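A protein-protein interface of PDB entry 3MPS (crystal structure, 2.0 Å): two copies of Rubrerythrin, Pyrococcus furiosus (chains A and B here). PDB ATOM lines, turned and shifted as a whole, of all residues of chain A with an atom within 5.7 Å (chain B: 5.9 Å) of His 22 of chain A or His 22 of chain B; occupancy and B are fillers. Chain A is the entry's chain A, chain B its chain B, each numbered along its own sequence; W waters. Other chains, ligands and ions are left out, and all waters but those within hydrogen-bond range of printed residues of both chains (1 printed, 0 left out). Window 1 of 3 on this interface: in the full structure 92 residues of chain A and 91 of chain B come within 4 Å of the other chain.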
ATOM      1  N   GLY A  17      12.735 -19.938 -24.644  1.00  0.00           N
ATOM      2  CA  GLY A  17      12.738 -20.613 -23.337  1.00  0.00           C
ATOM      3  C   GLY A  17      12.915 -19.639 -22.185  1.00  0.00           C
ATOM      4  O   GLY A  17      12.329 -19.824 -21.113  1.00  0.00           O
ATOM      5  N   GLU A  18      13.725 -18.601 -22.406  1.00  0.00           N
ATOM      6  CA  GLU A  18      13.894 -17.535 -21.407  1.00  0.00           C
ATOM      7  C   GLU A  18      12.724 -16.563 -21.422  1.00  0.00           C
ATOM      8  O   GLU A  18      12.412 -15.953 -20.407  1.00  0.00           O
ATOM      9  CB  GLU A  18      15.214 -16.781 -21.575  1.00  0.00           C
ATOM     10  CG  GLU A  18      16.476 -17.673 -21.433  1.00  0.00           C
ATOM     11  CD  GLU A  18      16.761 -18.129 -20.004  1.00  0.00           C
ATOM     12  OE1 GLU A  18      17.964 -18.238 -19.654  1.00  0.00           O
ATOM     13  OE2 GLU A  18      15.805 -18.370 -19.227  1.00  0.00           O
ATOM     14  N   SER A  19      12.121 -16.387 -22.590  1.00  0.00           N
ATOM     15  CA  SER A  19      10.893 -15.618 -22.685  1.00  0.00           C
ATOM     16  C   SER A  19       9.805 -16.264 -21.828  1.00  0.00           C
ATOM     17  O   SER A  19       9.127 -15.592 -21.063  1.00  0.00           O
ATOM     18  CB  SER A  19      10.476 -15.472 -24.151  1.00  0.00           C
ATOM     19  OG  SER A  19      11.470 -14.726 -24.855  1.00  0.00           O
ATOM     20  N   MET A  20       9.674 -17.576 -21.929  1.00  0.00           N
ATOM     21  CA  MET A  20       8.622 -18.294 -21.216  1.00  0.00           C
ATOM     22  C   MET A  20       8.874 -18.376 -19.713  1.00  0.00           C
ATOM     23  O   MET A  20       7.927 -18.348 -18.947  1.00  0.00           O
ATOM     24  CB  MET A  20       8.382 -19.677 -21.827  1.00  0.00           C
ATOM     25  CG  MET A  20       7.595 -19.643 -23.130  1.00  0.00           C
ATOM     26  SD  MET A  20       7.239 -21.297 -23.725  1.00  0.00           S
ATOM     27  CE  MET A  20       8.803 -21.665 -24.477  1.00  0.00           C
ATOM     28  N   ALA A  21      10.140 -18.462 -19.301  1.00  0.00           N
ATOM     29  CA  ALA A  21      10.506 -18.497 -17.882  1.00  0.00           C
ATOM     30  C   ALA A  21      10.241 -17.126 -17.276  1.00  0.00           C
ATOM     31  O   ALA A  21       9.619 -17.018 -16.225  1.00  0.00           O
ATOM     32  CB  ALA A  21      11.984 -18.891 -17.684  1.00  0.00           C
ATOM     33  N   HIS A  22      10.707 -16.082 -17.957  1.00  0.00           N
ATOM     34  CA  HIS A  22      10.433 -14.717 -17.530  1.00  0.00           C
ATOM     35  C   HIS A  22       8.938 -14.511 -17.323  1.00  0.00           C
ATOM     36  O   HIS A  22       8.526 -13.963 -16.310  1.00  0.00           O
ATOM     37  CB  HIS A  22      10.935 -13.751 -18.603  1.00  0.00           C
ATOM     38  CG  HIS A  22      10.434 -12.355 -18.442  1.00  0.00           C
ATOM     39  ND1 HIS A  22      11.056 -11.436 -17.631  1.00  0.00           N
ATOM     40  CD2 HIS A  22       9.386 -11.713 -19.006  1.00  0.00           C
ATOM     41  CE1 HIS A  22      10.414 -10.285 -17.699  1.00  0.00           C
ATOM     42  NE2 HIS A  22       9.392 -10.428 -18.523  1.00  0.00           N
ATOM     43  N   MET A  23       8.140 -14.975 -18.286  1.00  0.00           N
ATOM     44  CA  MET A  23       6.674 -14.825 -18.239  1.00  0.00           C
ATOM     45  C   MET A  23       6.053 -15.609 -17.080  1.00  0.00           C
ATOM     46  O   MET A  23       5.289 -15.039 -16.287  1.00  0.00           O
ATOM     47  CB  MET A  23       6.051 -15.257 -19.574  1.00  0.00           C
ATOM     48  CG  MET A  23       4.534 -15.071 -19.671  1.00  0.00           C
ATOM     49  SD  MET A  23       4.000 -13.371 -19.419  1.00  0.00           S
ATOM     50  CE  MET A  23       4.498 -12.607 -20.970  1.00  0.00           C
ATOM     51  N   ARG A  24       6.385 -16.901 -16.982  1.00  0.00           N
ATOM     52  CA  ARG A  24       5.920 -17.725 -15.859  1.00  0.00           C
ATOM     53  C   ARG A  24       6.162 -16.984 -14.553  1.00  0.00           C
ATOM     54  O   ARG A  24       5.227 -16.771 -13.796  1.00  0.00           O
ATOM     55  CB  ARG A  24       6.573 -19.122 -15.822  1.00  0.00           C
ATOM     56  CG  ARG A  24       6.183 -20.067 -16.978  1.00  0.00           C
ATOM     57  CD  ARG A  24       6.665 -21.540 -16.775  1.00  0.00           C
ATOM     58  NE  ARG A  24       8.091 -21.694 -16.452  1.00  0.00           N
ATOM     59  CZ  ARG A  24       9.066 -21.893 -17.343  1.00  0.00           C
ATOM     60  NH1 ARG A  24      10.322 -22.008 -16.924  1.00  0.00           N
ATOM     61  NH2 ARG A  24       8.799 -21.984 -18.643  1.00  0.00           N
ATOM     62  N   TYR A  25       7.406 -16.552 -14.321  1.00  0.00           N
ATOM     63  CA  TYR A  25       7.798 -15.901 -13.063  1.00  0.00           C
ATOM     64  C   TYR A  25       7.013 -14.630 -12.772  1.00  0.00           C
ATOM     65  O   TYR A  25       6.740 -14.323 -11.611  1.00  0.00           O
ATOM     66  CB  TYR A  25       9.305 -15.624 -13.014  1.00  0.00           C
ATOM     67  CG  TYR A  25      10.194 -16.858 -13.133  1.00  0.00           C
ATOM     68  CD1 TYR A  25      11.522 -16.739 -13.549  1.00  0.00           C
ATOM     69  CD2 TYR A  25       9.701 -18.148 -12.849  1.00  0.00           C
ATOM     70  CE1 TYR A  25      12.348 -17.864 -13.673  1.00  0.00           C
ATOM     71  CE2 TYR A  25      10.518 -19.276 -12.980  1.00  0.00           C
ATOM     72  CZ  TYR A  25      11.838 -19.121 -13.386  1.00  0.00           C
ATOM     73  OH  TYR A  25      12.658 -20.222 -13.506  1.00  0.00           O
ATOM     74  N   LEU A  26       6.645 -13.898 -13.827  1.00  0.00           N
ATOM     75  CA  LEU A  26       5.777 -12.723 -13.703  1.00  0.00           C
ATOM     76  C   LEU A  26       4.380 -13.119 -13.244  1.00  0.00           C
ATOM     77  O   LEU A  26       3.797 -12.479 -12.355  1.00  0.00           O
ATOM     78  CB  LEU A  26       5.682 -11.976 -15.035  1.00  0.00           C
ATOM     79  CG  LEU A  26       6.902 -11.269 -15.612  1.00  0.00           C
ATOM     80  CD1 LEU A  26       6.525 -10.558 -16.899  1.00  0.00           C
ATOM     81  CD2 LEU A  26       7.532 -10.286 -14.610  1.00  0.00           C
ATOM     82  N   ILE A  27       3.849 -14.172 -13.866  1.00  0.00           N
ATOM     83  CA  ILE A  27       2.554 -14.743 -13.511  1.00  0.00           C
ATOM     84  C   ILE A  27       2.601 -15.303 -12.077  1.00  0.00           C
ATOM     85  O   ILE A  27       1.664 -15.104 -11.294  1.00  0.00           O
ATOM     86  CB  ILE A  27       2.107 -15.856 -14.526  1.00  0.00           C
ATOM     87  CG1 ILE A  27       1.891 -15.277 -15.927  1.00  0.00           C
ATOM     88  CG2 ILE A  27       0.848 -16.579 -14.024  1.00  0.00           C
ATOM     89  CD1 ILE A  27       1.869 -16.334 -17.094  1.00  0.00           C
ATOM     90  N   ALA A  48      12.721 -12.870 -12.739  1.00  0.00           N
ATOM     91  CA  ALA A  48      12.123 -12.597 -14.039  1.00  0.00           C
ATOM     92  C   ALA A  48      13.005 -11.615 -14.838  1.00  0.00           C
ATOM     93  O   ALA A  48      13.233 -11.817 -16.033  1.00  0.00           O
ATOM     94  CB  ALA A  48      10.712 -12.066 -13.884  1.00  0.00           C
ATOM     95  N   TYR A  49      13.516 -10.576 -14.170  1.00  0.00           N
ATOM     96  CA  TYR A  49      14.466  -9.635 -14.809  1.00  0.00           C
ATOM     97  C   TYR A  49      15.804 -10.303 -15.195  1.00  0.00           C
ATOM     98  O   TYR A  49      16.377  -9.978 -16.227  1.00  0.00           O
ATOM     99  CB  TYR A  49      14.705  -8.371 -13.953  1.00  0.00           C
ATOM    100  CG  TYR A  49      15.696  -7.382 -14.589  1.00  0.00           C
ATOM    101  CD1 TYR A  49      15.314  -6.549 -15.644  1.00  0.00           C
ATOM    102  CD2 TYR A  49      17.023  -7.300 -14.133  1.00  0.00           C
ATOM    103  CE1 TYR A  49      16.227  -5.655 -16.230  1.00  0.00           C
ATOM    104  CE2 TYR A  49      17.942  -6.417 -14.711  1.00  0.00           C
ATOM    105  CZ  TYR A  49      17.543  -5.606 -15.752  1.00  0.00           C
ATOM    106  OH  TYR A  49      18.452  -4.744 -16.304  1.00  0.00           O
ATOM    107  N   GLU A  51      16.111 -13.317 -16.275  1.00  0.00           N
ATOM    108  CA  GLU A  51      15.783 -14.010 -17.538  1.00  0.00           C
ATOM    109  C   GLU A  51      15.570 -13.048 -18.708  1.00  0.00           C
ATOM    110  O   GLU A  51      15.774 -13.413 -19.861  1.00  0.00           O
ATOM    111  CB  GLU A  51      14.544 -14.895 -17.399  1.00  0.00           C
ATOM    112  CG  GLU A  51      14.518 -15.923 -16.213  1.00  0.00           C
ATOM    113  CD  GLU A  51      15.814 -16.706 -15.967  1.00  0.00           C
ATOM    114  OE1 GLU A  51      16.036 -17.030 -14.786  1.00  0.00           O
ATOM    115  OE2 GLU A  51      16.592 -17.040 -16.895  1.00  0.00           O
ATOM    116  N   PHE A  52      15.113 -11.836 -18.413  1.00  0.00           N
ATOM    117  CA  PHE A  52      15.031 -10.796 -19.440  1.00  0.00           C
ATOM    118  C   PHE A  52      16.436 -10.525 -19.982  1.00  0.00           C
ATOM    119  O   PHE A  52      16.632 -10.410 -21.203  1.00  0.00           O
ATOM    120  CB  PHE A  52      14.365  -9.525 -18.883  1.00  0.00           C
ATOM    121  CG  PHE A  52      14.762  -8.252 -19.599  1.00  0.00           C
ATOM    122  CD1 PHE A  52      14.087  -7.831 -20.738  1.00  0.00           C
ATOM    123  CD2 PHE A  52      15.796  -7.464 -19.109  1.00  0.00           C
ATOM    124  CE1 PHE A  52      14.464  -6.643 -21.403  1.00  0.00           C
ATOM    125  CE2 PHE A  52      16.177  -6.281 -19.761  1.00  0.00           C
ATOM    126  CZ  PHE A  52      15.514  -5.878 -20.912  1.00  0.00           C
ATOM    127  N   GLY B  17       4.612 -17.809 -28.045  1.00  0.00           N
ATOM    128  CA  GLY B  17       4.571 -16.657 -28.945  1.00  0.00           C
ATOM    129  C   GLY B  17       4.315 -15.357 -28.207  1.00  0.00           C
ATOM    130  O   GLY B  17       4.918 -14.318 -28.524  1.00  0.00           O
ATOM    131  N   GLU B  18       3.426 -15.400 -27.222  1.00  0.00           N
ATOM    132  CA  GLU B  18       3.098 -14.181 -26.463  1.00  0.00           C
ATOM    133  C   GLU B  18       4.160 -13.830 -25.453  1.00  0.00           C
ATOM    134  O   GLU B  18       4.328 -12.673 -25.133  1.00  0.00           O
ATOM    135  CB  GLU B  18       1.734 -14.251 -25.791  1.00  0.00           C
ATOM    136  CG  GLU B  18       0.568 -14.215 -26.762  1.00  0.00           C
ATOM    137  CD  GLU B  18       0.381 -12.852 -27.441  1.00  0.00           C
ATOM    138  OE1 GLU B  18       1.380 -12.174 -27.748  1.00  0.00           O
ATOM    139  OE2 GLU B  18      -0.763 -12.477 -27.704  1.00  0.00           O
ATOM    140  N   SER B  19       4.856 -14.846 -24.949  1.00  0.00           N
ATOM    141  CA  SER B  19       6.051 -14.664 -24.125  1.00  0.00           C
ATOM    142  C   SER B  19       7.173 -13.950 -24.913  1.00  0.00           C
ATOM    143  O   SER B  19       7.770 -12.981 -24.419  1.00  0.00           O
ATOM    144  CB  SER B  19       6.526 -16.013 -23.581  1.00  0.00           C
ATOM    145  OG  SER B  19       5.539 -16.576 -22.713  1.00  0.00           O
ATOM    146  N   MET B  20       7.445 -14.414 -26.123  1.00  0.00           N
ATOM    147  CA  MET B  20       8.477 -13.799 -26.969  1.00  0.00           C
ATOM    148  C   MET B  20       8.119 -12.366 -27.386  1.00  0.00           C
ATOM    149  O   MET B  20       8.972 -11.485 -27.368  1.00  0.00           O
ATOM    150  CB  MET B  20       8.795 -14.677 -28.183  1.00  0.00           C
ATOM    151  CG  MET B  20       9.558 -15.955 -27.825  1.00  0.00           C
ATOM    152  SD  MET B  20      10.168 -16.901 -29.242  1.00  0.00           S
ATOM    153  CE  MET B  20       8.675 -17.735 -29.723  1.00  0.00           C
ATOM    154  N   ALA B  21       6.862 -12.135 -27.748  1.00  0.00           N
ATOM    155  CA  ALA B  21       6.362 -10.775 -28.031  1.00  0.00           C
ATOM    156  C   ALA B  21       6.539  -9.820 -26.837  1.00  0.00           C
ATOM    157  O   ALA B  21       7.116  -8.751 -26.989  1.00  0.00           O
ATOM    158  CB  ALA B  21       4.867 -10.823 -28.482  1.00  0.00           C
ATOM    159  N   HIS B  22       6.026 -10.209 -25.667  1.00  0.00           N
ATOM    160  CA  HIS B  22       6.207  -9.472 -24.419  1.00  0.00           C
ATOM    161  C   HIS B  22       7.691  -9.127 -24.243  1.00  0.00           C
ATOM    162  O   HIS B  22       8.055  -7.946 -24.045  1.00  0.00           O
ATOM    163  CB  HIS B  22       5.690 -10.314 -23.228  1.00  0.00           C
ATOM    164  CG  HIS B  22       6.118  -9.817 -21.878  1.00  0.00           C
ATOM    165  ND1 HIS B  22       5.342  -8.975 -21.107  1.00  0.00           N
ATOM    166  CD2 HIS B  22       7.212 -10.096 -21.131  1.00  0.00           C
ATOM    167  CE1 HIS B  22       5.955  -8.730 -19.964  1.00  0.00           C
ATOM    168  NE2 HIS B  22       7.089  -9.405 -19.949  1.00  0.00           N
ATOM    169  N   MET B  23       8.531 -10.157 -24.357  1.00  0.00           N
ATOM    170  CA  MET B  23       9.984 -10.018 -24.195  1.00  0.00           C
ATOM    171  C   MET B  23      10.612  -9.046 -25.213  1.00  0.00           C
ATOM    172  O   MET B  23      11.365  -8.151 -24.819  1.00  0.00           O
ATOM    173  CB  MET B  23      10.673 -11.391 -24.243  1.00  0.00           C
ATOM    174  CG  MET B  23      12.190 -11.366 -23.951  1.00  0.00           C
ATOM    175  SD  MET B  23      12.586 -10.619 -22.341  1.00  0.00           S
ATOM    176  CE  MET B  23      12.261 -12.047 -21.286  1.00  0.00           C
ATOM    177  N   ARG B  24      10.317  -9.232 -26.496  1.00  0.00           N
ATOM    178  CA  ARG B  24      10.803  -8.323 -27.554  1.00  0.00           C
ATOM    179  C   ARG B  24      10.425  -6.854 -27.265  1.00  0.00           C
ATOM    180  O   ARG B  24      11.248  -5.945 -27.443  1.00  0.00           O
ATOM    181  CB  ARG B  24      10.262  -8.722 -28.929  1.00  0.00           C
ATOM    182  CG  ARG B  24      10.801 -10.027 -29.516  1.00  0.00           C
ATOM    183  CD  ARG B  24      10.578 -10.107 -31.022  1.00  0.00           C
ATOM    184  NE  ARG B  24       9.178 -10.377 -31.376  1.00  0.00           N
ATOM    185  CZ  ARG B  24       8.623 -11.593 -31.384  1.00  0.00           C
ATOM    186  NH1 ARG B  24       7.346 -11.735 -31.712  1.00  0.00           N
ATOM    187  NH2 ARG B  24       9.345 -12.668 -31.077  1.00  0.00           N
ATOM    188  N   TYR B  25       9.200  -6.637 -26.789  1.00  0.00           N
ATOM    189  CA  TYR B  25       8.715  -5.292 -26.520  1.00  0.00           C
ATOM    190  C   TYR B  25       9.353  -4.624 -25.300  1.00  0.00           C
ATOM    191  O   TYR B  25       9.577  -3.402 -25.312  1.00  0.00           O
ATOM    192  CB  TYR B  25       7.177  -5.243 -26.451  1.00  0.00           C
ATOM    193  CG  TYR B  25       6.452  -5.728 -27.703  1.00  0.00           C
ATOM    194  CD1 TYR B  25       5.120  -6.154 -27.630  1.00  0.00           C
ATOM    195  CD2 TYR B  25       7.093  -5.768 -28.950  1.00  0.00           C
ATOM    196  CE1 TYR B  25       4.440  -6.607 -28.758  1.00  0.00           C
ATOM    197  CE2 TYR B  25       6.429  -6.236 -30.089  1.00  0.00           C
ATOM    198  CZ  TYR B  25       5.093  -6.648 -29.985  1.00  0.00           C
ATOM    199  OH  TYR B  25       4.412  -7.087 -31.095  1.00  0.00           O
ATOM    200  N   LEU B  26       9.643  -5.400 -24.248  1.00  0.00           N
ATOM    201  CA  LEU B  26      10.492  -4.906 -23.153  1.00  0.00           C
ATOM    202  C   LEU B  26      11.890  -4.477 -23.640  1.00  0.00           C
ATOM    203  O   LEU B  26      12.426  -3.456 -23.195  1.00  0.00           O
ATOM    204  CB  LEU B  26      10.653  -5.951 -22.040  1.00  0.00           C
ATOM    205  CG  LEU B  26       9.419  -6.397 -21.254  1.00  0.00           C
ATOM    206  CD1 LEU B  26       9.868  -7.298 -20.101  1.00  0.00           C
ATOM    207  CD2 LEU B  26       8.639  -5.200 -20.739  1.00  0.00           C
ATOM    208  N   ILE B  27      12.474  -5.280 -24.527  1.00  0.00           N
ATOM    209  CA  ILE B  27      13.805  -5.024 -25.076  1.00  0.00           C
ATOM    210  C   ILE B  27      13.763  -3.785 -25.976  1.00  0.00           C
ATOM    211  O   ILE B  27      14.662  -2.943 -25.929  1.00  0.00           O
ATOM    212  CB  ILE B  27      14.329  -6.222 -25.920  1.00  0.00           C
ATOM    213  CG1 ILE B  27      14.490  -7.482 -25.061  1.00  0.00           C
ATOM    214  CG2 ILE B  27      15.632  -5.832 -26.643  1.00  0.00           C
ATOM    215  CD1 ILE B  27      14.848  -8.754 -25.858  1.00  0.00           C
ATOM    216  N   ALA B  48       3.440  -4.611 -24.059  1.00  0.00           N
ATOM    217  CA  ALA B  48       4.111  -5.741 -23.430  1.00  0.00           C
ATOM    218  C   ALA B  48       3.227  -6.347 -22.344  1.00  0.00           C
ATOM    219  O   ALA B  48       3.013  -7.560 -22.332  1.00  0.00           O
ATOM    220  CB  ALA B  48       5.443  -5.312 -22.845  1.00  0.00           C
ATOM    221  N   TYR B  49       2.721  -5.495 -21.448  1.00  0.00           N
ATOM    222  CA  TYR B  49       1.755  -5.917 -20.421  1.00  0.00           C
ATOM    223  C   TYR B  49       0.495  -6.546 -21.005  1.00  0.00           C
ATOM    224  O   TYR B  49      -0.021  -7.498 -20.434  1.00  0.00           O
ATOM    225  CB  TYR B  49       1.368  -4.776 -19.460  1.00  0.00           C
ATOM    226  CG  TYR B  49       0.325  -5.215 -18.451  1.00  0.00           C
ATOM    227  CD1 TYR B  49       0.681  -5.935 -17.316  1.00  0.00           C
ATOM    228  CD2 TYR B  49      -1.031  -4.954 -18.666  1.00  0.00           C
ATOM    229  CE1 TYR B  49      -0.299  -6.357 -16.393  1.00  0.00           C
ATOM    230  CE2 TYR B  49      -1.998  -5.374 -17.769  1.00  0.00           C
ATOM    231  CZ  TYR B  49      -1.631  -6.081 -16.641  1.00  0.00           C
ATOM    232  OH  TYR B  49      -2.614  -6.494 -15.761  1.00  0.00           O
ATOM    233  N   GLU B  51       0.383  -8.276 -23.722  1.00  0.00           N
ATOM    234  CA  GLU B  51       0.867  -9.621 -24.061  1.00  0.00           C
ATOM    235  C   GLU B  51       0.971 -10.573 -22.862  1.00  0.00           C
ATOM    236  O   GLU B  51       0.637 -11.746 -22.975  1.00  0.00           O
ATOM    237  CB  GLU B  51       2.172  -9.548 -24.836  1.00  0.00           C
ATOM    238  CG  GLU B  51       2.145  -8.580 -26.012  1.00  0.00           C
ATOM    239  CD  GLU B  51       0.947  -8.741 -26.941  1.00  0.00           C
ATOM    240  OE1 GLU B  51       0.374  -9.849 -27.071  1.00  0.00           O
ATOM    241  OE2 GLU B  51       0.591  -7.739 -27.590  1.00  0.00           O
ATOM    242  N   PHE B  52       1.438 -10.062 -21.727  1.00  0.00           N
ATOM    243  CA  PHE B  52       1.413 -10.798 -20.455  1.00  0.00           C
ATOM    244  C   PHE B  52      -0.010 -11.258 -20.068  1.00  0.00           C
ATOM    245  O   PHE B  52      -0.186 -12.336 -19.467  1.00  0.00           O
ATOM    246  CB  PHE B  52       2.044  -9.934 -19.346  1.00  0.00           C
ATOM    247  CG  PHE B  52       1.547 -10.243 -17.952  1.00  0.00           C
ATOM    248  CD1 PHE B  52       2.228 -11.140 -17.145  1.00  0.00           C
ATOM    249  CD2 PHE B  52       0.396  -9.619 -17.447  1.00  0.00           C
ATOM    250  CE1 PHE B  52       1.778 -11.442 -15.855  1.00  0.00           C
ATOM    251  CE2 PHE B  52      -0.062  -9.906 -16.162  1.00  0.00           C
ATOM    252  CZ  PHE B  52       0.629 -10.822 -15.368  1.00  0.00           C
HETATM  253  O   HOH W   1       8.486 -13.133 -21.634  1.00  0.00           O
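A ring nitrogen (NE2) of His 22 of chain A lies within hydrogen-bond range of a ring nitrogen (NE2) of His 22 of chain B (2.9 Å).
A ring nitrogen (ND1) of His 22 of chain A sits at hydrogen-bond distance from the backbone carbonyl oxygen (O) of Ala 48 of chain A, 2.7 Å away.
A ring nitrogen (ND1) of His 22 of chain B sits at hydrogen-bond distance from the backbone carbonyl oxygen (O) of Ala 48 of chain B (3.0 Å).
CB of Ser 19 of chain B touches O of Ser 19 of chain A (3.6 Å).
Ser 19 of chain A touches Met 20 of chain B (OG to CG, 3.7 Å).
CG of His 22 of chain A touches CE of Met 23 of chain B (3.4 Å).
Leu 26 of chain B touches His 22 of chain A (CD1 to NE2, 3.5 Å).
Ser 19 of chain B touches Met 23 of chain A (OG to CB, 3.4 Å).
CE of Met 23 of chain A touches CG of His 22 of chain B, at 3.4 Å.
CE of Met 23 of chain A touches CA of Phe 52 of chain B (3.6 Å).
CD1 of Leu 26 of chain A touches NE2 of His 22 of chain B (3.3 Å).
Met 23 of chain B touches Phe 52 of chain A (SD to CD1, 3.5 Å).
Ile 27 of chain B touches Phe 52 of chain A (CG1 to CE1, 3.8 Å).
Of chain B, only His 22, Met 23 and Leu 26 come within 4 Å of His 22 of chain A.
Of chain A, only His 22, Met 23 and Leu 26 come within 4 Å of His 22 of chain B.
Of the printed residues of chain A, Ser 19 of chain B touches Ser 19 (3.6 Å), Met 20 (3.7 Å) and Met 23 (3.4 Å).
Of the printed residues of chain B, Ser 19 of chain A touches Ser 19, Met 20 and Met 23.
Of the printed residues of chain B, Met 23 of chain A touches Ser 19, His 22 and Phe 52.
The nearest residue of chain B that does not touch His 22 of chain A is Ser 19 of chain B (5.8 Å).
The nearest printed residue of chain A that does not touch His 22 of chain B is Ser 19 of chain A (5.8 Å).
Of the 15 printed residues of chain B, 7 touch a printed residue of chain A.
Along chain B the printed residues that touch a printed residue of chain A span positions 19 to 52.
Printed residues of chain A that touch a printed residue of chain B: Ser 19, Met 20, His 22, Met 23, Leu 26, Ile 27 and Phe 52.
Among the printed residues, 15 pairs touch across the chains.
Ser 19 of chain A touches Met 20 of chain B, and with the chains exchanged Met 20 of chain A touches Ser 19 of chain B.
His 22 of chain B touches its own counterpart, His 22 of chain A.
His 22 of chain A touches Met 23 of chain B, and with the chains exchanged Met 23 of chain A touches His 22 of chain B.
His 22 of chain A touches Leu 26 of chain B, and with the chains exchanged Leu 26 of chain A touches His 22 of chain B.
Positions printed for both chains: 17, 18, 19, 20, 21, 22, 23, 24, 25, 26, 27, 48, 49, 51 and 52.
Water W1 bridges the backbone carbonyl oxygen of Ser 19 of chain A (2.6 Å) and the backbone carbonyl oxygen of Ser 19 of chain B (2.9 Å).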
